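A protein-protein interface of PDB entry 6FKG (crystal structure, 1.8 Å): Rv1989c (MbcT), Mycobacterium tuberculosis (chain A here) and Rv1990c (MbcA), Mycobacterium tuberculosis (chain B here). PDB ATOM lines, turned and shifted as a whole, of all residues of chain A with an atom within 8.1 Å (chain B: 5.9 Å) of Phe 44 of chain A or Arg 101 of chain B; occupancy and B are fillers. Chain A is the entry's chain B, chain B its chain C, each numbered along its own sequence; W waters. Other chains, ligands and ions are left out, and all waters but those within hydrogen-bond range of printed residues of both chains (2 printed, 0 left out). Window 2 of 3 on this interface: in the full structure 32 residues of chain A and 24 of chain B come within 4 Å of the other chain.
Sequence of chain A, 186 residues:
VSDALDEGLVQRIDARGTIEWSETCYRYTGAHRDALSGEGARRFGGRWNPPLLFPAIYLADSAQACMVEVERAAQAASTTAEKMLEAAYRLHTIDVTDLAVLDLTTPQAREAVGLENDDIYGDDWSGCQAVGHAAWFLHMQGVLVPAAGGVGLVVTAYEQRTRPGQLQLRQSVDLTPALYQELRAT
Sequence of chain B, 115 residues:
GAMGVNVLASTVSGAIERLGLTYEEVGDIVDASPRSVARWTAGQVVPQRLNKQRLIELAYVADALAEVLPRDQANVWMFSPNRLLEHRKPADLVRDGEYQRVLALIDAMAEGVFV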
ATOM      1  N   GLY A  38     -11.016 -28.049 -24.812  1.00  0.00           N
ATOM      2  CA  GLY A  38     -10.060 -26.977 -25.056  1.00  0.00           C
ATOM      3  C   GLY A  38     -10.706 -25.606 -25.169  1.00  0.00           C
ATOM      4  O   GLY A  38     -10.109 -24.664 -25.691  1.00  0.00           O
ATOM      5  N   GLU A  39     -11.926 -25.487 -24.659  1.00  0.00           N
ATOM      6  CA  GLU A  39     -12.700 -24.265 -24.851  1.00  0.00           C
ATOM      7  C   GLU A  39     -12.183 -23.077 -24.028  1.00  0.00           C
ATOM      8  O   GLU A  39     -12.394 -21.936 -24.410  1.00  0.00           O
ATOM      9  CB  GLU A  39     -14.150 -24.515 -24.525  1.00  0.00           C
ATOM     10  CG  GLU A  39     -14.726 -25.611 -25.383  1.00  0.00           C
ATOM     11  CD  GLU A  39     -14.748 -25.246 -26.860  1.00  0.00           C
ATOM     12  OE1 GLU A  39     -14.842 -24.037 -27.182  1.00  0.00           O
ATOM     13  OE2 GLU A  39     -14.660 -26.181 -27.691  1.00  0.00           O
ATOM     14  N   GLY A  40     -11.524 -23.350 -22.910  1.00  0.00           N
ATOM     15  CA  GLY A  40     -11.034 -22.283 -22.055  1.00  0.00           C
ATOM     16  C   GLY A  40      -9.923 -21.501 -22.734  1.00  0.00           C
ATOM     17  O   GLY A  40      -9.894 -20.256 -22.704  1.00  0.00           O
ATOM     18  N   ALA A  41      -9.003 -22.236 -23.347  1.00  0.00           N
ATOM     19  CA  ALA A  41      -7.933 -21.627 -24.117  1.00  0.00           C
ATOM     20  C   ALA A  41      -8.508 -20.841 -25.290  1.00  0.00           C
ATOM     21  O   ALA A  41      -7.978 -19.799 -25.665  1.00  0.00           O
ATOM     22  CB  ALA A  41      -6.957 -22.691 -24.603  1.00  0.00           C
ATOM     23  N   ARG A  42      -9.601 -21.325 -25.871  1.00  0.00           N
ATOM     24  CA  ARG A  42     -10.239 -20.576 -26.950  1.00  0.00           C
ATOM     25  C   ARG A  42     -10.883 -19.283 -26.444  1.00  0.00           C
ATOM     26  O   ARG A  42     -10.813 -18.247 -27.098  1.00  0.00           O
ATOM     27  CB  ARG A  42     -11.300 -21.423 -27.656  1.00  0.00           C
ATOM     28  CG  ARG A  42     -11.976 -20.708 -28.803  1.00  0.00           C
ATOM     29  CD  ARG A  42     -13.264 -21.405 -29.201  1.00  0.00           C
ATOM     30  NE  ARG A  42     -13.342 -21.570 -30.640  1.00  0.00           N
ATOM     31  CZ  ARG A  42     -14.033 -22.530 -31.247  1.00  0.00           C
ATOM     32  NH1 ARG A  42     -14.727 -23.412 -30.531  1.00  0.00           N
ATOM     33  NH2 ARG A  42     -14.026 -22.605 -32.573  1.00  0.00           N
ATOM     34  N   ARG A  43     -11.532 -19.350 -25.286  1.00  0.00           N
ATOM     35  CA  ARG A  43     -12.240 -18.189 -24.780  1.00  0.00           C
ATOM     36  C   ARG A  43     -11.271 -17.071 -24.361  1.00  0.00           C
ATOM     37  O   ARG A  43     -11.522 -15.899 -24.649  1.00  0.00           O
ATOM     38  CB  ARG A  43     -13.145 -18.599 -23.612  1.00  0.00           C
ATOM     39  CG  ARG A  43     -14.527 -19.060 -24.080  1.00  0.00           C
ATOM     40  CD  ARG A  43     -15.300 -19.814 -23.010  1.00  0.00           C
ATOM     41  NE  ARG A  43     -15.450 -19.048 -21.777  1.00  0.00           N
ATOM     42  CZ  ARG A  43     -16.440 -18.197 -21.523  1.00  0.00           C
ATOM     43  NH1 ARG A  43     -17.391 -17.985 -22.427  1.00  0.00           N
ATOM     44  NH2 ARG A  43     -16.481 -17.566 -20.354  1.00  0.00           N
ATOM     45  N   PHE A  44     -10.175 -17.444 -23.706  1.00  0.00           N
ATOM     46  CA  PHE A  44      -9.247 -16.454 -23.131  1.00  0.00           C
ATOM     47  C   PHE A  44      -7.999 -16.249 -23.965  1.00  0.00           C
ATOM     48  O   PHE A  44      -7.398 -15.169 -23.939  1.00  0.00           O
ATOM     49  CB  PHE A  44      -8.821 -16.855 -21.706  1.00  0.00           C
ATOM     50  CG  PHE A  44      -8.051 -15.768 -20.991  1.00  0.00           C
ATOM     51  CD1 PHE A  44      -8.691 -14.592 -20.623  1.00  0.00           C
ATOM     52  CD2 PHE A  44      -6.693 -15.906 -20.731  1.00  0.00           C
ATOM     53  CE1 PHE A  44      -8.009 -13.570 -20.000  1.00  0.00           C
ATOM     54  CE2 PHE A  44      -5.984 -14.872 -20.092  1.00  0.00           C
ATOM     55  CZ  PHE A  44      -6.643 -13.713 -19.733  1.00  0.00           C
ATOM     56  N   GLY A  45      -7.612 -17.277 -24.713  1.00  0.00           N
ATOM     57  CA  GLY A  45      -6.276 -17.326 -25.280  1.00  0.00           C
ATOM     58  C   GLY A  45      -5.365 -18.075 -24.324  1.00  0.00           C
ATOM     59  O   GLY A  45      -5.699 -18.241 -23.151  1.00  0.00           O
ATOM     60  N   GLY A  46      -4.220 -18.531 -24.827  1.00  0.00           N
ATOM     61  CA  GLY A  46      -3.196 -19.172 -24.014  1.00  0.00           C
ATOM     62  C   GLY A  46      -1.849 -18.712 -24.535  1.00  0.00           C
ATOM     63  O   GLY A  46      -1.794 -18.013 -25.547  1.00  0.00           O
ATOM     64  N   ARG A  47      -0.758 -19.079 -23.857  1.00  0.00           N
ATOM     65  CA  ARG A  47       0.542 -18.588 -24.280  1.00  0.00           C
ATOM     66  C   ARG A  47       0.779 -18.894 -25.755  1.00  0.00           C
ATOM     67  O   ARG A  47       1.313 -18.057 -26.489  1.00  0.00           O
ATOM     68  CB  ARG A  47       1.683 -19.180 -23.439  1.00  0.00           C
ATOM     69  CG  ARG A  47       3.060 -18.707 -23.941  1.00  0.00           C
ATOM     70  CD  ARG A  47       4.171 -18.898 -22.915  1.00  0.00           C
ATOM     71  NE  ARG A  47       3.942 -18.166 -21.666  1.00  0.00           N
ATOM     72  CZ  ARG A  47       4.380 -16.937 -21.395  1.00  0.00           C
ATOM     73  NH1 ARG A  47       5.095 -16.245 -22.282  1.00  0.00           N
ATOM     74  NH2 ARG A  47       4.103 -16.391 -20.216  1.00  0.00           N
ATOM     75  N   ASN A  49      -1.698 -19.834 -28.124  1.00  0.00           N
ATOM     76  CA  ASN A  49      -2.824 -19.711 -29.058  1.00  0.00           C
ATOM     77  C   ASN A  49      -3.571 -18.413 -28.871  1.00  0.00           C
ATOM     78  O   ASN A  49      -3.859 -18.009 -27.745  1.00  0.00           O
ATOM     79  CB  ASN A  49      -3.821 -20.884 -28.918  1.00  0.00           C
ATOM     80  CG  ASN A  49      -4.606 -20.835 -27.626  1.00  0.00           C
ATOM     81  OD1 ASN A  49      -4.092 -21.211 -26.571  1.00  0.00           O
ATOM     82  ND2 ASN A  49      -5.848 -20.356 -27.696  1.00  0.00           N
ATOM     83  N   PRO A  50      -3.909 -17.757 -29.986  1.00  0.00           N
ATOM     84  CA  PRO A  50      -4.785 -16.591 -29.887  1.00  0.00           C
ATOM     85  C   PRO A  50      -6.172 -17.076 -29.483  1.00  0.00           C
ATOM     86  O   PRO A  50      -6.474 -18.261 -29.662  1.00  0.00           O
ATOM     87  CB  PRO A  50      -4.784 -16.029 -31.308  1.00  0.00           C
ATOM     88  CG  PRO A  50      -4.625 -17.258 -32.162  1.00  0.00           C
ATOM     89  CD  PRO A  50      -3.688 -18.166 -31.385  1.00  0.00           C
ATOM     90  N   PRO A  51      -6.997 -16.180 -28.940  1.00  0.00           N
ATOM     91  CA  PRO A  51      -8.359 -16.554 -28.559  1.00  0.00           C
ATOM     92  C   PRO A  51      -9.293 -16.635 -29.763  1.00  0.00           C
ATOM     93  O   PRO A  51      -8.928 -16.174 -30.843  1.00  0.00           O
ATOM     94  CB  PRO A  51      -8.775 -15.429 -27.612  1.00  0.00           C
ATOM     95  CG  PRO A  51      -7.947 -14.249 -28.031  1.00  0.00           C
ATOM     96  CD  PRO A  51      -6.653 -14.802 -28.532  1.00  0.00           C
ATOM     97  N   LEU A  52     -10.448 -17.265 -29.564  1.00  0.00           N
ATOM     98  CA  LEU A  52     -11.603 -17.164 -30.463  1.00  0.00           C
ATOM     99  C   LEU A  52     -11.476 -17.845 -31.822  1.00  0.00           C
ATOM    100  O   LEU A  52     -12.336 -17.639 -32.683  1.00  0.00           O
ATOM    101  CB  LEU A  52     -11.953 -15.688 -30.707  1.00  0.00           C
ATOM    102  CG  LEU A  52     -12.113 -14.756 -29.503  1.00  0.00           C
ATOM    103  CD1 LEU A  52     -12.467 -13.345 -29.975  1.00  0.00           C
ATOM    104  CD2 LEU A  52     -13.157 -15.288 -28.536  1.00  0.00           C
ATOM    105  N   TRP A 125       2.622 -12.689 -24.697  1.00  0.00           N
ATOM    106  CA  TRP A 125       2.322 -13.928 -25.405  1.00  0.00           C
ATOM    107  C   TRP A 125       2.331 -13.788 -26.936  1.00  0.00           C
ATOM    108  O   TRP A 125       2.147 -14.787 -27.636  1.00  0.00           O
ATOM    109  CB  TRP A 125       0.940 -14.448 -24.984  1.00  0.00           C
ATOM    110  CG  TRP A 125       0.798 -14.972 -23.565  1.00  0.00           C
ATOM    111  CD1 TRP A 125       1.790 -15.143 -22.630  1.00  0.00           C
ATOM    112  CD2 TRP A 125      -0.425 -15.382 -22.932  1.00  0.00           C
ATOM    113  NE1 TRP A 125       1.252 -15.644 -21.459  1.00  0.00           N
ATOM    114  CE2 TRP A 125      -0.102 -15.801 -21.622  1.00  0.00           C
ATOM    115  CE3 TRP A 125      -1.763 -15.446 -23.352  1.00  0.00           C
ATOM    116  CZ2 TRP A 125      -1.069 -16.262 -20.730  1.00  0.00           C
ATOM    117  CZ3 TRP A 125      -2.719 -15.908 -22.467  1.00  0.00           C
ATOM    118  CH2 TRP A 125      -2.367 -16.311 -21.168  1.00  0.00           C
ATOM    119  N   GLN A 129       1.846 -16.827 -29.616  1.00  0.00           N
ATOM    120  CA  GLN A 129       0.486 -16.984 -30.148  1.00  0.00           C
ATOM    121  C   GLN A 129       0.464 -16.955 -31.671  1.00  0.00           C
ATOM    122  O   GLN A 129      -0.277 -17.706 -32.301  1.00  0.00           O
ATOM    123  CB  GLN A 129      -0.438 -15.901 -29.593  1.00  0.00           C
ATOM    124  CG  GLN A 129      -0.790 -16.109 -28.124  1.00  0.00           C
ATOM    125  CD  GLN A 129      -1.677 -15.009 -27.580  1.00  0.00           C
ATOM    126  OE1 GLN A 129      -1.483 -13.833 -27.888  1.00  0.00           O
ATOM    127  NE2 GLN A 129      -2.668 -15.385 -26.781  1.00  0.00           N
ATOM    128  N   LEU B  84      -2.208 -11.349 -16.303  1.00  0.00           N
ATOM    129  CA  LEU B  84      -2.964 -11.913 -17.423  1.00  0.00           C
ATOM    130  C   LEU B  84      -4.035 -10.942 -17.925  1.00  0.00           C
ATOM    131  O   LEU B  84      -4.596 -11.118 -19.018  1.00  0.00           O
ATOM    132  CB  LEU B  84      -3.601 -13.248 -17.019  1.00  0.00           C
ATOM    133  CG  LEU B  84      -2.579 -14.282 -16.538  1.00  0.00           C
ATOM    134  CD1 LEU B  84      -3.254 -15.600 -16.144  1.00  0.00           C
ATOM    135  CD2 LEU B  84      -1.528 -14.505 -17.608  1.00  0.00           C
ATOM    136  N   LEU B  85      -4.314  -9.915 -17.126  1.00  0.00           N
ATOM    137  CA  LEU B  85      -5.273  -8.883 -17.502  1.00  0.00           C
ATOM    138  C   LEU B  85      -4.570  -7.536 -17.658  1.00  0.00           C
ATOM    139  O   LEU B  85      -5.110  -6.501 -17.279  1.00  0.00           O
ATOM    140  CB  LEU B  85      -6.394  -8.784 -16.453  1.00  0.00           C
ATOM    141  CG  LEU B  85      -7.192 -10.052 -16.144  1.00  0.00           C
ATOM    142  CD1 LEU B  85      -8.121  -9.784 -14.977  1.00  0.00           C
ATOM    143  CD2 LEU B  85      -8.002 -10.542 -17.365  1.00  0.00           C
ATOM    144  N   GLU B  86      -3.358  -7.560 -18.213  1.00  0.00           N
ATOM    145  CA  GLU B  86      -2.559  -6.347 -18.400  1.00  0.00           C
ATOM    146  C   GLU B  86      -2.376  -5.590 -17.074  1.00  0.00           C
ATOM    147  O   GLU B  86      -2.430  -4.358 -17.021  1.00  0.00           O
ATOM    148  CB  GLU B  86      -3.200  -5.447 -19.466  1.00  0.00           C
ATOM    149  CG  GLU B  86      -3.341  -6.111 -20.849  1.00  0.00           C
ATOM    150  CD  GLU B  86      -4.459  -7.149 -20.910  1.00  0.00           C
ATOM    151  OE1 GLU B  86      -5.575  -6.848 -20.437  1.00  0.00           O
ATOM    152  OE2 GLU B  86      -4.223  -8.269 -21.417  1.00  0.00           O
ATOM    153  N   ARG B  88      -4.231  -5.379 -14.475  1.00  0.00           N
ATOM    154  CA  ARG B  88      -5.421  -4.761 -13.904  1.00  0.00           C
ATOM    155  C   ARG B  88      -6.066  -5.704 -12.890  1.00  0.00           C
ATOM    156  O   ARG B  88      -5.831  -6.906 -12.916  1.00  0.00           O
ATOM    157  CB  ARG B  88      -6.420  -4.390 -15.012  1.00  0.00           C
ATOM    158  CG  ARG B  88      -5.926  -3.283 -15.939  1.00  0.00           C
ATOM    159  CD  ARG B  88      -6.903  -3.050 -17.092  1.00  0.00           C
ATOM    160  NE  ARG B  88      -6.972  -4.223 -17.960  1.00  0.00           N
ATOM    161  CZ  ARG B  88      -7.998  -4.510 -18.759  1.00  0.00           C
ATOM    162  NH1 ARG B  88      -9.057  -3.709 -18.805  1.00  0.00           N
ATOM    163  NH2 ARG B  88      -7.965  -5.606 -19.512  1.00  0.00           N
ATOM    164  N   LEU B  93     -12.127  -4.566 -13.662  1.00  0.00           N
ATOM    165  CA  LEU B  93     -12.744  -4.979 -14.928  1.00  0.00           C
ATOM    166  C   LEU B  93     -14.250  -5.138 -14.767  1.00  0.00           C
ATOM    167  O   LEU B  93     -15.036  -4.722 -15.638  1.00  0.00           O
ATOM    168  CB  LEU B  93     -12.129  -6.287 -15.451  1.00  0.00           C
ATOM    169  CG  LEU B  93     -10.956  -6.082 -16.422  1.00  0.00           C
ATOM    170  CD1 LEU B  93      -9.733  -5.564 -15.672  1.00  0.00           C
ATOM    171  CD2 LEU B  93     -10.634  -7.369 -17.182  1.00  0.00           C
ATOM    172  N   GLU B  98     -16.245  -5.077 -18.034  1.00  0.00           N
ATOM    173  CA  GLU B  98     -15.495  -6.134 -18.715  1.00  0.00           C
ATOM    174  C   GLU B  98     -15.557  -7.475 -17.987  1.00  0.00           C
ATOM    175  O   GLU B  98     -14.587  -8.241 -18.005  1.00  0.00           O
ATOM    176  CB  GLU B  98     -14.034  -5.702 -18.897  1.00  0.00           C
ATOM    177  CG  GLU B  98     -13.889  -4.424 -19.694  1.00  0.00           C
ATOM    178  CD  GLU B  98     -12.479  -3.868 -19.670  1.00  0.00           C
ATOM    179  OE1 GLU B  98     -11.524  -4.642 -19.880  1.00  0.00           O
ATOM    180  OE2 GLU B  98     -12.330  -2.657 -19.423  1.00  0.00           O
ATOM    181  N   TYR B  99     -16.696  -7.775 -17.360  1.00  0.00           N
ATOM    182  CA  TYR B  99     -16.835  -9.038 -16.639  1.00  0.00           C
ATOM    183  C   TYR B  99     -16.638 -10.257 -17.555  1.00  0.00           C
ATOM    184  O   TYR B  99     -16.222 -11.314 -17.094  1.00  0.00           O
ATOM    185  CB  TYR B  99     -18.208  -9.138 -15.948  1.00  0.00           C
ATOM    186  CG  TYR B  99     -19.334  -9.519 -16.886  1.00  0.00           C
ATOM    187  CD1 TYR B  99     -19.868  -8.584 -17.775  1.00  0.00           C
ATOM    188  CD2 TYR B  99     -19.849 -10.811 -16.903  1.00  0.00           C
ATOM    189  CE1 TYR B  99     -20.873  -8.916 -18.632  1.00  0.00           C
ATOM    190  CE2 TYR B  99     -20.873 -11.157 -17.784  1.00  0.00           C
ATOM    191  CZ  TYR B  99     -21.376 -10.199 -18.637  1.00  0.00           C
ATOM    192  OH  TYR B  99     -22.389 -10.497 -19.518  1.00  0.00           O
ATOM    193  N   GLN B 100     -16.930 -10.118 -18.845  1.00  0.00           N
ATOM    194  CA  GLN B 100     -16.820 -11.276 -19.736  1.00  0.00           C
ATOM    195  C   GLN B 100     -15.369 -11.731 -19.826  1.00  0.00           C
ATOM    196  O   GLN B 100     -15.095 -12.930 -19.844  1.00  0.00           O
ATOM    197  CB  GLN B 100     -17.383 -10.959 -21.124  1.00  0.00           C
ATOM    198  CG  GLN B 100     -18.897 -11.072 -21.205  1.00  0.00           C
ATOM    199  CD  GLN B 100     -19.373 -12.522 -21.210  1.00  0.00           C
ATOM    200  OE1 GLN B 100     -18.567 -13.458 -21.220  1.00  0.00           O
ATOM    201  NE2 GLN B 100     -20.686 -12.712 -21.217  1.00  0.00           N
ATOM    202  N   ARG B 101     -14.443 -10.774 -19.848  1.00  0.00           N
ATOM    203  CA  ARG B 101     -13.020 -11.110 -19.911  1.00  0.00           C
ATOM    204  C   ARG B 101     -12.593 -11.835 -18.651  1.00  0.00           C
ATOM    205  O   ARG B 101     -11.773 -12.758 -18.691  1.00  0.00           O
ATOM    206  CB  ARG B 101     -12.161  -9.846 -20.097  1.00  0.00           C
ATOM    207  CG  ARG B 101     -10.645 -10.122 -20.159  1.00  0.00           C
ATOM    208  CD  ARG B 101     -10.163 -10.202 -21.593  1.00  0.00           C
ATOM    209  NE  ARG B 101      -8.775 -10.643 -21.738  1.00  0.00           N
ATOM    210  CZ  ARG B 101      -7.701  -9.899 -21.464  1.00  0.00           C
ATOM    211  NH1 ARG B 101      -7.834  -8.655 -20.998  1.00  0.00           N
ATOM    212  NH2 ARG B 101      -6.483 -10.409 -21.639  1.00  0.00           N
ATOM    213  N   VAL B 102     -13.128 -11.392 -17.515  1.00  0.00           N
ATOM    214  CA  VAL B 102     -12.838 -12.039 -16.239  1.00  0.00           C
ATOM    215  C   VAL B 102     -13.362 -13.480 -16.217  1.00  0.00           C
ATOM    216  O   VAL B 102     -12.676 -14.398 -15.773  1.00  0.00           O
ATOM    217  CB  VAL B 102     -13.445 -11.243 -15.061  1.00  0.00           C
ATOM    218  CG1 VAL B 102     -13.130 -11.936 -13.741  1.00  0.00           C
ATOM    219  CG2 VAL B 102     -12.925  -9.798 -15.069  1.00  0.00           C
ATOM    220  N   LEU B 103     -14.591 -13.685 -16.684  1.00  0.00           N
ATOM    221  CA  LEU B 103     -15.140 -15.037 -16.796  1.00  0.00           C
ATOM    222  C   LEU B 103     -14.304 -15.912 -17.731  1.00  0.00           C
ATOM    223  O   LEU B 103     -14.129 -17.116 -17.479  1.00  0.00           O
ATOM    224  CB  LEU B 103     -16.590 -15.001 -17.300  1.00  0.00           C
ATOM    225  CG  LEU B 103     -17.608 -14.368 -16.340  1.00  0.00           C
ATOM    226  CD1 LEU B 103     -19.021 -14.402 -16.956  1.00  0.00           C
ATOM    227  CD2 LEU B 103     -17.582 -15.079 -14.980  1.00  0.00           C
ATOM    228  N   ALA B 104     -13.806 -15.317 -18.812  1.00  0.00           N
ATOM    229  CA  ALA B 104     -12.980 -16.065 -19.756  1.00  0.00           C
ATOM    230  C   ALA B 104     -11.666 -16.488 -19.084  1.00  0.00           C
ATOM    231  O   ALA B 104     -11.233 -17.648 -19.223  1.00  0.00           O
ATOM    232  CB  ALA B 104     -12.715 -15.237 -21.035  1.00  0.00           C
ATOM    233  N   LEU B 105     -11.042 -15.576 -18.336  1.00  0.00           N
ATOM    234  CA  LEU B 105      -9.832 -15.946 -17.584  1.00  0.00           C
ATOM    235  C   LEU B 105     -10.123 -17.089 -16.581  1.00  0.00           C
ATOM    236  O   LEU B 105      -9.363 -18.045 -16.486  1.00  0.00           O
ATOM    237  CB  LEU B 105      -9.239 -14.727 -16.854  1.00  0.00           C
ATOM    238  CG  LEU B 105      -8.077 -15.030 -15.889  1.00  0.00           C
ATOM    239  CD1 LEU B 105      -6.971 -15.807 -16.581  1.00  0.00           C
ATOM    240  CD2 LEU B 105      -7.511 -13.750 -15.275  1.00  0.00           C
ATOM    241  N   ILE B 106     -11.238 -17.015 -15.860  1.00  0.00           N
ATOM    242  CA  ILE B 106     -11.598 -18.075 -14.910  1.00  0.00           C
ATOM    243  C   ILE B 106     -11.770 -19.421 -15.620  1.00  0.00           C
ATOM    244  O   ILE B 106     -11.318 -20.469 -15.139  1.00  0.00           O
ATOM    245  CB  ILE B 106     -12.866 -17.679 -14.122  1.00  0.00           C
ATOM    246  CG1 ILE B 106     -12.520 -16.522 -13.176  1.00  0.00           C
ATOM    247  CG2 ILE B 106     -13.464 -18.868 -13.365  1.00  0.00           C
ATOM    248  CD1 ILE B 106     -13.757 -15.776 -12.619  1.00  0.00           C
ATOM    249  N   ALA B 108     -10.216 -20.323 -18.374  1.00  0.00           N
ATOM    250  CA  ALA B 108      -8.860 -20.757 -18.705  1.00  0.00           C
ATOM    251  C   ALA B 108      -8.169 -21.353 -17.474  1.00  0.00           C
ATOM    252  O   ALA B 108      -7.495 -22.367 -17.572  1.00  0.00           O
ATOM    253  CB  ALA B 108      -8.030 -19.588 -19.296  1.00  0.00           C
HETATM  254  O   HOH W   1      -5.302 -13.343 -23.081  1.00  0.00           O
HETATM  255  O   HOH W   2      -8.665 -12.667 -23.483  1.00  0.00           O
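The guanidinium group of Arg 101 of chain B sits at hydrogen-bond distance from the backbone carbonyl oxygen of Leu 84 of chain B (3.3 Å).
The side-chain carboxylate (OE1) of Glu 86 of chain B lies within salt-bridge range of the guanidinium group (NH1) of Arg 101 of chain B, 2.9 Å away.
Among the printed residues, merely in contact across the chains: Phe 44 of chain A with Leu 84 of chain B (3.4 Å), Phe 44 of chain A with Leu 105 of chain B (3.4 Å), Phe 44 of chain A with Arg 101 of chain B (3.5 Å), Phe 44 of chain A with Ala 104 of chain B (3.6 Å), Trp 125 of chain A with Leu 84 of chain B (3.6 Å), Phe 44 of chain A with Ala 108 of chain B (3.7 Å), Arg 43 of chain A with Leu 103 of chain B (3.7 Å), Arg 43 of chain A with Ala 104 of chain B (3.8 Å) and Gly 40 of chain A with Ala 108 of chain B (3.9 Å).
Printed residues of chain B within 4 Å of Phe 44 of chain A: Leu 84 (3.4 Å), Arg 101 (3.5 Å), Ala 104 (3.6 Å), Leu 105 (3.4 Å) and Ala 108 (3.7 Å).
Of chain A, only Phe 44 (3.5 Å) comes within 4 Å of Arg 101 of chain B.
Of chain A, only Arg 43 (3.8 Å) and Phe 44 (3.6 Å) come within 4 Å of Ala 104 of chain B.
Of the printed residues of chain A, Leu 84 of chain B touches Phe 44 (3.4 Å) and Trp 125 (3.6 Å).
Of the printed residues of chain A, Leu 105 of chain B touches Phe 44 (3.4 Å).
Leu 93 of chain B touches none of the printed residues of chain A.
The nearest printed residue of chain B that does not touch Phe 44 of chain A is Leu 85 of chain B (4.01 Å).
The nearest residue of chain A that does not touch Arg 101 of chain B is Arg 43 of chain A (6.6 Å).
Printed residues of chain A that touch a printed residue of chain B: Gly 40, Arg 43, Phe 44 and Trp 125.
Hydrophobic or aromatic side chains of chain A within 4 Å of the printed part of chain B: Phe 44 and Trp 125.
Printed residues of chain B that touch a printed residue of chain A: Leu 84, Arg 101, Leu 103, Ala 104, Leu 105 and Ala 108.
Among the printed residues, 9 pairs touch across the chains.
Water W2 lies within hydrogen-bond range of the guanidinium group of Arg 101 of chain B and the backbone carbonyl oxygen of Phe 44 of chain A.
Water W1 lies within hydrogen-bond range of O of Phe 44 of chain A and NH2 of Arg 101 of chain B.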
